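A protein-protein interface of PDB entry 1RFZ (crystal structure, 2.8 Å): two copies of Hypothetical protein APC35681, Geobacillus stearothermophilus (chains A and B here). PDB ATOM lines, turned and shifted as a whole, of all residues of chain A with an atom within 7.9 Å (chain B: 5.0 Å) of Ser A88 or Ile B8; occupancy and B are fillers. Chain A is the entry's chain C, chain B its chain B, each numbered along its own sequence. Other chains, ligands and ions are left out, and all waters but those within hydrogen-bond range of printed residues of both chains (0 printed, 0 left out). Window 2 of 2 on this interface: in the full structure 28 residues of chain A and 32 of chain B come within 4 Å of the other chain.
No position is printed for both chains. Of the 8 pairs that touch across the chains among the printed residues, none has its exchanged pair printed and touching as well.
Hydrophobic or aromatic side chains of chain B within 4 Å of the printed part of chain A: Ile B8, Met B9 and Leu B12. Of the 18 printed residues of chain A, 5 touch a printed residue of chain B. Hydrophobic or aromatic side chains of chain A that line the printed part of chain B: Pro A85, Ile A89 and Leu A96. Among the printed residues, 8 pairs touch across the chains.
The side-chain carboxylate of Glu A84 sits at hydrogen-bond distance from the side-chain hydroxyl of Ser A88 (3.0 Å). The backbone carbonyl oxygen (O) of Pro A85 lies within hydrogen-bond range of the side-chain hydroxyl (OG) of Ser A88, at 3.0 Å. The backbone carbonyl oxygen (O) of Ile A89 is in hydrogen-bond range of the backbone NH (N) of Glu A94 (3.0 Å).
OG of Ser B5 is in hydrogen-bond range of OE2 of Glu A94 (2.8 Å).
Of chain B, only Ile B8 (3.9 Å) comes within 4 Å of Ser A88. Of chain A, only Ser A88 and Ile A89 come within 4 Å of Ile B8. Of the printed residues of chain B, Glu A94 touches Ser B5 and Met B9. Of the printed residues of chain B, Pro A85 touches Leu B12. Of the printed residues of chain A, Ser B5 touches Glu A94 (2.8 Å). Printed residues of chain B within 4 Å of Ile A89: Ile B8 (3.7 Å), Met B9 (3.8 Å) and Leu B12 (3.6 Å). Of the printed residues of chain A, Met B9 touches Ile A89, Glu A94 and Leu A96. The nearest residue of chain A that does not touch Ile B8 is Pro A85 (4.4 Å). The nearest printed residue of chain B that does not touch Leu A96 is Asn B10 (5.2 Å).
Pro A85 touches Leu B12. CD1 of Ile B8 touches OG of Ser A88, at 3.9 Å. Ile B8 touches Ile A89. CD1 of Ile A89 touches SD of Met B9 (3.8 Å). Ile A89 touches Leu B12 (CD1 to CD2, 3.6 Å). Met B9 touches Glu A94. Leu A96 touches Met B9 (C to CE, 3.5 Å).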
ATOM      1  N   ALA A  77      30.290   4.576 -13.509  1.00  0.00           N
ATOM      2  CA  ALA A  77      30.959   4.020 -12.344  1.00  0.00           C
ATOM      3  C   ALA A  77      32.359   3.475 -12.659  1.00  0.00           C
ATOM      4  O   ALA A  77      33.318   3.831 -11.984  1.00  0.00           O
ATOM      5  CB  ALA A  77      30.114   2.929 -11.729  1.00  0.00           C
ATOM      6  N   GLY A  80      34.769   5.967 -13.081  1.00  0.00           N
ATOM      7  CA  GLY A  80      34.871   6.797 -11.887  1.00  0.00           C
ATOM      8  C   GLY A  80      34.348   8.217 -12.063  1.00  0.00           C
ATOM      9  O   GLY A  80      34.952   9.182 -11.577  1.00  0.00           O
ATOM     10  N   LEU A  82      30.993   9.124 -11.292  1.00  0.00           N
ATOM     11  CA  LEU A  82      29.833   9.416 -10.470  1.00  0.00           C
ATOM     12  C   LEU A  82      30.316  10.178  -9.257  1.00  0.00           C
ATOM     13  O   LEU A  82      31.521  10.392  -9.121  1.00  0.00           O
ATOM     14  CB  LEU A  82      29.135   8.128 -10.040  1.00  0.00           C
ATOM     15  CG  LEU A  82      28.516   7.290 -11.169  1.00  0.00           C
ATOM     16  CD1 LEU A  82      27.838   6.056 -10.569  1.00  0.00           C
ATOM     17  CD2 LEU A  82      27.515   8.104 -11.941  1.00  0.00           C
ATOM     18  N   ASP A  83      29.394  10.600  -8.392  1.00  0.00           N
ATOM     19  CA  ASP A  83      29.752  11.333  -7.173  1.00  0.00           C
ATOM     20  C   ASP A  83      29.767  10.435  -5.949  1.00  0.00           C
ATOM     21  O   ASP A  83      28.896   9.575  -5.782  1.00  0.00           O
ATOM     22  CB  ASP A  83      28.782  12.486  -6.942  1.00  0.00           C
ATOM     23  CG  ASP A  83      29.098  13.679  -7.812  1.00  0.00           C
ATOM     24  OD1 ASP A  83      30.245  14.179  -7.703  1.00  0.00           O
ATOM     25  OD2 ASP A  83      28.219  14.115  -8.598  1.00  0.00           O
ATOM     26  N   GLU A  84      30.762  10.614  -5.093  1.00  0.00           N
ATOM     27  CA  GLU A  84      30.838   9.796  -3.893  1.00  0.00           C
ATOM     28  C   GLU A  84      29.698  10.216  -2.988  1.00  0.00           C
ATOM     29  O   GLU A  84      29.305  11.383  -3.011  1.00  0.00           O
ATOM     30  CB  GLU A  84      32.170  10.018  -3.183  1.00  0.00           C
ATOM     31  CG  GLU A  84      33.353   9.432  -3.906  1.00  0.00           C
ATOM     32  CD  GLU A  84      33.264   7.924  -4.046  1.00  0.00           C
ATOM     33  OE1 GLU A  84      34.214   7.320  -4.590  1.00  0.00           O
ATOM     34  OE2 GLU A  84      32.243   7.343  -3.611  1.00  0.00           O
ATOM     35  N   PRO A  85      29.144   9.283  -2.183  1.00  0.00           N
ATOM     36  CA  PRO A  85      29.540   7.878  -2.095  1.00  0.00           C
ATOM     37  C   PRO A  85      28.856   6.945  -3.114  1.00  0.00           C
ATOM     38  O   PRO A  85      29.178   5.752  -3.155  1.00  0.00           O
ATOM     39  CB  PRO A  85      29.191   7.522  -0.635  1.00  0.00           C
ATOM     40  CG  PRO A  85      27.954   8.302  -0.405  1.00  0.00           C
ATOM     41  CD  PRO A  85      28.291   9.646  -1.035  1.00  0.00           C
ATOM     42  N   LEU A  86      27.923   7.480  -3.921  1.00  0.00           N
ATOM     43  CA  LEU A  86      27.197   6.674  -4.936  1.00  0.00           C
ATOM     44  C   LEU A  86      28.190   5.925  -5.816  1.00  0.00           C
ATOM     45  O   LEU A  86      28.005   4.743  -6.121  1.00  0.00           O
ATOM     46  CB  LEU A  86      26.343   7.561  -5.851  1.00  0.00           C
ATOM     47  CG  LEU A  86      24.900   7.197  -6.272  1.00  0.00           C
ATOM     48  CD1 LEU A  86      24.624   7.849  -7.615  1.00  0.00           C
ATOM     49  CD2 LEU A  86      24.685   5.726  -6.375  1.00  0.00           C
ATOM     50  N   GLN A  87      29.226   6.647  -6.233  1.00  0.00           N
ATOM     51  CA  GLN A  87      30.306   6.116  -7.052  1.00  0.00           C
ATOM     52  C   GLN A  87      30.819   4.781  -6.503  1.00  0.00           C
ATOM     53  O   GLN A  87      30.832   3.771  -7.197  1.00  0.00           O
ATOM     54  CB  GLN A  87      31.450   7.142  -7.114  1.00  0.00           C
ATOM     55  CG  GLN A  87      32.771   6.612  -7.624  1.00  0.00           C
ATOM     56  CD  GLN A  87      32.671   6.042  -9.022  1.00  0.00           C
ATOM     57  OE1 GLN A  87      32.351   6.751  -9.978  1.00  0.00           O
ATOM     58  NE2 GLN A  87      32.942   4.749  -9.148  1.00  0.00           N
ATOM     59  N   SER A  88      31.236   4.755  -5.254  1.00  0.00           N
ATOM     60  CA  SER A  88      31.722   3.495  -4.736  1.00  0.00           C
ATOM     61  C   SER A  88      30.580   2.496  -4.532  1.00  0.00           C
ATOM     62  O   SER A  88      30.721   1.325  -4.852  1.00  0.00           O
ATOM     63  CB  SER A  88      32.532   3.711  -3.445  1.00  0.00           C
ATOM     64  OG  SER A  88      31.887   4.601  -2.553  1.00  0.00           O
ATOM     65  N   ILE A  89      29.443   2.952  -4.030  1.00  0.00           N
ATOM     66  CA  ILE A  89      28.331   2.041  -3.821  1.00  0.00           C
ATOM     67  C   ILE A  89      28.007   1.252  -5.088  1.00  0.00           C
ATOM     68  O   ILE A  89      27.849   0.020  -5.041  1.00  0.00           O
ATOM     69  CB  ILE A  89      27.069   2.783  -3.386  1.00  0.00           C
ATOM     70  CG1 ILE A  89      27.288   3.401  -2.005  1.00  0.00           C
ATOM     71  CG2 ILE A  89      25.869   1.842  -3.417  1.00  0.00           C
ATOM     72  CD1 ILE A  89      26.086   4.184  -1.472  1.00  0.00           C
ATOM     73  N   ILE A  90      27.905   1.947  -6.221  1.00  0.00           N
ATOM     74  CA  ILE A  90      27.583   1.268  -7.479  1.00  0.00           C
ATOM     75  C   ILE A  90      28.765   0.423  -7.995  1.00  0.00           C
ATOM     76  O   ILE A  90      28.592  -0.742  -8.392  1.00  0.00           O
ATOM     77  CB  ILE A  90      27.109   2.302  -8.566  1.00  0.00           C
ATOM     78  CG1 ILE A  90      25.731   2.862  -8.171  1.00  0.00           C
ATOM     79  CG2 ILE A  90      27.073   1.640  -9.973  1.00  0.00           C
ATOM     80  CD1 ILE A  90      25.158   3.797  -9.185  1.00  0.00           C
ATOM     81  N   ARG A  91      29.960   1.005  -7.953  1.00  0.00           N
ATOM     82  CA  ARG A  91      31.168   0.324  -8.408  1.00  0.00           C
ATOM     83  C   ARG A  91      31.424  -0.973  -7.644  1.00  0.00           C
ATOM     84  O   ARG A  91      31.823  -1.985  -8.228  1.00  0.00           O
ATOM     85  CB  ARG A  91      32.376   1.259  -8.261  1.00  0.00           C
ATOM     86  CG  ARG A  91      33.662   0.722  -8.850  1.00  0.00           C
ATOM     87  CD  ARG A  91      33.474   0.319 -10.300  1.00  0.00           C
ATOM     88  NE  ARG A  91      34.056  -0.989 -10.588  1.00  0.00           N
ATOM     89  CZ  ARG A  91      35.077  -1.181 -11.418  1.00  0.00           C
ATOM     90  NH1 ARG A  91      35.634  -0.149 -12.043  1.00  0.00           N
ATOM     91  NH2 ARG A  91      35.542  -2.403 -11.635  1.00  0.00           N
ATOM     92  N   ARG A  92      31.199  -0.937  -6.338  1.00  0.00           N
ATOM     93  CA  ARG A  92      31.407  -2.095  -5.486  1.00  0.00           C
ATOM     94  C   ARG A  92      30.215  -3.032  -5.477  1.00  0.00           C
ATOM     95  O   ARG A  92      30.219  -4.047  -4.781  1.00  0.00           O
ATOM     96  CB  ARG A  92      31.711  -1.639  -4.060  1.00  0.00           C
ATOM     97  CG  ARG A  92      33.070  -0.997  -3.912  1.00  0.00           C
ATOM     98  CD  ARG A  92      34.179  -2.019  -4.140  1.00  0.00           C
ATOM     99  NE  ARG A  92      35.505  -1.404  -4.091  1.00  0.00           N
ATOM    100  CZ  ARG A  92      36.639  -2.067  -3.878  1.00  0.00           C
ATOM    101  NH1 ARG A  92      36.621  -3.382  -3.690  1.00  0.00           N
ATOM    102  NH2 ARG A  92      37.794  -1.411  -3.846  1.00  0.00           N
ATOM    103  N   ASP A  93      29.190  -2.704  -6.246  1.00  0.00           N
ATOM    104  CA  ASP A  93      27.996  -3.542  -6.274  1.00  0.00           C
ATOM    105  C   ASP A  93      27.446  -3.812  -4.845  1.00  0.00           C
ATOM    106  O   ASP A  93      27.047  -4.924  -4.511  1.00  0.00           O
ATOM    107  CB  ASP A  93      28.320  -4.854  -6.996  1.00  0.00           C
ATOM    108  CG  ASP A  93      27.096  -5.705  -7.240  1.00  0.00           C
ATOM    109  OD1 ASP A  93      26.384  -6.033  -6.273  1.00  0.00           O
ATOM    110  OD2 ASP A  93      26.836  -6.064  -8.401  1.00  0.00           O
ATOM    111  N   GLU A  94      27.425  -2.789  -4.000  1.00  0.00           N
ATOM    112  CA  GLU A  94      26.921  -2.945  -2.640  1.00  0.00           C
ATOM    113  C   GLU A  94      25.588  -3.685  -2.536  1.00  0.00           C
ATOM    114  O   GLU A  94      24.543  -3.183  -2.959  1.00  0.00           O
ATOM    115  CB  GLU A  94      26.756  -1.584  -1.981  1.00  0.00           C
ATOM    116  CG  GLU A  94      28.037  -0.971  -1.502  1.00  0.00           C
ATOM    117  CD  GLU A  94      28.865  -1.935  -0.672  1.00  0.00           C
ATOM    118  OE1 GLU A  94      28.275  -2.842  -0.032  1.00  0.00           O
ATOM    119  OE2 GLU A  94      30.110  -1.766  -0.658  1.00  0.00           O
ATOM    120  N   LEU A  96      23.445  -3.991  -0.252  1.00  0.00           N
ATOM    121  CA  LEU A  96      22.336  -3.302   0.393  1.00  0.00           C
ATOM    122  C   LEU A  96      21.747  -2.158  -0.438  1.00  0.00           C
ATOM    123  O   LEU A  96      20.805  -1.483  -0.004  1.00  0.00           O
ATOM    124  CB  LEU A  96      22.758  -2.784   1.768  1.00  0.00           C
ATOM    125  CG  LEU A  96      22.784  -3.797   2.919  1.00  0.00           C
ATOM    126  CD1 LEU A  96      23.122  -3.121   4.242  1.00  0.00           C
ATOM    127  CD2 LEU A  96      21.417  -4.476   2.981  1.00  0.00           C
ATOM    128  N   CYS A 141      32.488  -2.729 -14.566  1.00  0.00           N
ATOM    129  CA  CYS A 141      31.328  -2.648 -13.680  1.00  0.00           C
ATOM    130  C   CYS A 141      30.053  -3.119 -14.388  1.00  0.00           C
ATOM    131  O   CYS A 141      29.645  -2.557 -15.404  1.00  0.00           O
ATOM    132  CB  CYS A 141      31.103  -1.212 -13.189  1.00  0.00           C
ATOM    133  SG  CYS A 141      29.729  -1.105 -11.995  1.00  0.00           S
ATOM    134  N   THR A 143      27.275  -3.847 -12.337  1.00  0.00           N
ATOM    135  CA  THR A 143      26.372  -3.838 -11.204  1.00  0.00           C
ATOM    136  C   THR A 143      24.930  -3.897 -11.682  1.00  0.00           C
ATOM    137  O   THR A 143      24.128  -4.634 -11.114  1.00  0.00           O
ATOM    138  CB  THR A 143      26.561  -2.580 -10.365  1.00  0.00           C
ATOM    139  OG1 THR A 143      27.826  -2.645  -9.705  1.00  0.00           O
ATOM    140  CG2 THR A 143      25.456  -2.442  -9.332  1.00  0.00           C
ATOM    141  N   MET B   4      34.222  -1.319   5.422  1.00  0.00           N
ATOM    142  CA  MET B   4      34.062  -0.046   4.732  1.00  0.00           C
ATOM    143  C   MET B   4      32.672  -0.001   4.089  1.00  0.00           C
ATOM    144  O   MET B   4      32.069   1.056   3.914  1.00  0.00           O
ATOM    145  CB  MET B   4      35.147   0.077   3.663  1.00  0.00           C
ATOM    146  CG  MET B   4      35.062   1.335   2.854  1.00  0.00           C
ATOM    147  SD  MET B   4      35.274   2.879   3.978  1.00  0.00           S
ATOM    148  CE  MET B   4      36.164   4.060   2.724  1.00  0.00           C
ATOM    149  N   SER B   5      32.172  -1.175   3.734  1.00  0.00           N
ATOM    150  CA  SER B   5      30.857  -1.286   3.133  1.00  0.00           C
ATOM    151  C   SER B   5      29.812  -0.996   4.202  1.00  0.00           C
ATOM    152  O   SER B   5      28.845  -0.290   3.948  1.00  0.00           O
ATOM    153  CB  SER B   5      30.671  -2.685   2.538  1.00  0.00           C
ATOM    154  OG  SER B   5      31.576  -2.878   1.461  1.00  0.00           O
ATOM    155  N   GLU B   6      30.019  -1.534   5.399  1.00  0.00           N
ATOM    156  CA  GLU B   6      29.094  -1.300   6.499  1.00  0.00           C
ATOM    157  C   GLU B   6      29.090   0.177   6.832  1.00  0.00           C
ATOM    158  O   GLU B   6      28.041   0.799   6.981  1.00  0.00           O
ATOM    159  CB  GLU B   6      29.504  -2.098   7.738  1.00  0.00           C
ATOM    160  CG  GLU B   6      29.150  -3.565   7.662  1.00  0.00           C
ATOM    161  CD  GLU B   6      29.415  -4.292   8.959  1.00  0.00           C
ATOM    162  OE1 GLU B   6      28.970  -3.797  10.018  1.00  0.00           O
ATOM    163  OE2 GLU B   6      30.061  -5.363   8.916  1.00  0.00           O
ATOM    164  N   PHE B   7      30.276   0.744   6.946  1.00  0.00           N
ATOM    165  CA  PHE B   7      30.382   2.148   7.257  1.00  0.00           C
ATOM    166  C   PHE B   7      29.619   2.975   6.214  1.00  0.00           C
ATOM    167  O   PHE B   7      28.930   3.940   6.552  1.00  0.00           O
ATOM    168  CB  PHE B   7      31.858   2.563   7.306  1.00  0.00           C
ATOM    169  CG  PHE B   7      32.061   4.040   7.339  1.00  0.00           C
ATOM    170  CD1 PHE B   7      31.675   4.784   8.450  1.00  0.00           C
ATOM    171  CD2 PHE B   7      32.574   4.702   6.231  1.00  0.00           C
ATOM    172  CE1 PHE B   7      31.794   6.175   8.452  1.00  0.00           C
ATOM    173  CE2 PHE B   7      32.701   6.102   6.221  1.00  0.00           C
ATOM    174  CZ  PHE B   7      32.309   6.839   7.335  1.00  0.00           C
ATOM    175  N   ILE B   8      29.722   2.596   4.948  1.00  0.00           N
ATOM    176  CA  ILE B   8      29.037   3.349   3.909  1.00  0.00           C
ATOM    177  C   ILE B   8      27.513   3.187   3.866  1.00  0.00           C
ATOM    178  O   ILE B   8      26.780   4.177   3.866  1.00  0.00           O
ATOM    179  CB  ILE B   8      29.634   3.036   2.514  1.00  0.00           C
ATOM    180  CG1 ILE B   8      31.066   3.589   2.462  1.00  0.00           C
ATOM    181  CG2 ILE B   8      28.760   3.648   1.402  1.00  0.00           C
ATOM    182  CD1 ILE B   8      31.787   3.426   1.128  1.00  0.00           C
ATOM    183  N   MET B   9      27.035   1.952   3.852  1.00  0.00           N
ATOM    184  CA  MET B   9      25.606   1.713   3.771  1.00  0.00           C
ATOM    185  C   MET B   9      24.863   2.120   5.029  1.00  0.00           C
ATOM    186  O   MET B   9      23.621   2.133   5.081  1.00  0.00           O
ATOM    187  CB  MET B   9      25.352   0.243   3.426  1.00  0.00           C
ATOM    188  CG  MET B   9      25.877  -0.144   2.037  1.00  0.00           C
ATOM    189  SD  MET B   9      25.391   1.122   0.606  1.00  0.00           S
ATOM    190  CE  MET B   9      23.483   0.719   0.568  1.00  0.00           C
ATOM    191  N   ASN B  10      25.634   2.482   6.045  1.00  0.00           N
ATOM    192  CA  ASN B  10      25.063   2.891   7.314  1.00  0.00           C
ATOM    193  C   ASN B  10      25.082   4.393   7.442  1.00  0.00           C
ATOM    194  O   ASN B  10      24.416   4.951   8.299  1.00  0.00           O
ATOM    195  CB  ASN B  10      25.833   2.242   8.454  1.00  0.00           C
ATOM    196  CG  ASN B  10      25.419   0.798   8.681  1.00  0.00           C
ATOM    197  OD1 ASN B  10      25.208   0.038   7.734  1.00  0.00           O
ATOM    198  ND2 ASN B  10      25.304   0.411   9.944  1.00  0.00           N
ATOM    199  N   ASN B  11      25.817   5.060   6.565  1.00  0.00           N
ATOM    200  CA  ASN B  11      25.889   6.503   6.635  1.00  0.00           C
ATOM    201  C   ASN B  11      25.539   7.197   5.333  1.00  0.00           C
ATOM    202  O   ASN B  11      26.361   7.951   4.793  1.00  0.00           O
ATOM    203  CB  ASN B  11      27.285   6.947   7.077  1.00  0.00           C
ATOM    204  CG  ASN B  11      27.644   6.441   8.453  1.00  0.00           C
ATOM    205  OD1 ASN B  11      28.014   5.289   8.615  1.00  0.00           O
ATOM    206  ND2 ASN B  11      27.524   7.296   9.452  1.00  0.00           N
ATOM    207  N   LEU B  12      24.321   6.960   4.838  1.00  0.00           N
ATOM    208  CA  LEU B  12      23.862   7.591   3.602  1.00  0.00           C
ATOM    209  C   LEU B  12      22.889   8.741   3.874  1.00  0.00           C
ATOM    210  O   LEU B  12      22.850   9.720   3.132  1.00  0.00           O
ATOM    211  CB  LEU B  12      23.208   6.544   2.689  1.00  0.00           C
ATOM    212  CG  LEU B  12      24.146   5.449   2.148  1.00  0.00           C
ATOM    213  CD1 LEU B  12      23.394   4.487   1.228  1.00  0.00           C
ATOM    214  CD2 LEU B  12      25.307   6.111   1.410  1.00  0.00           C
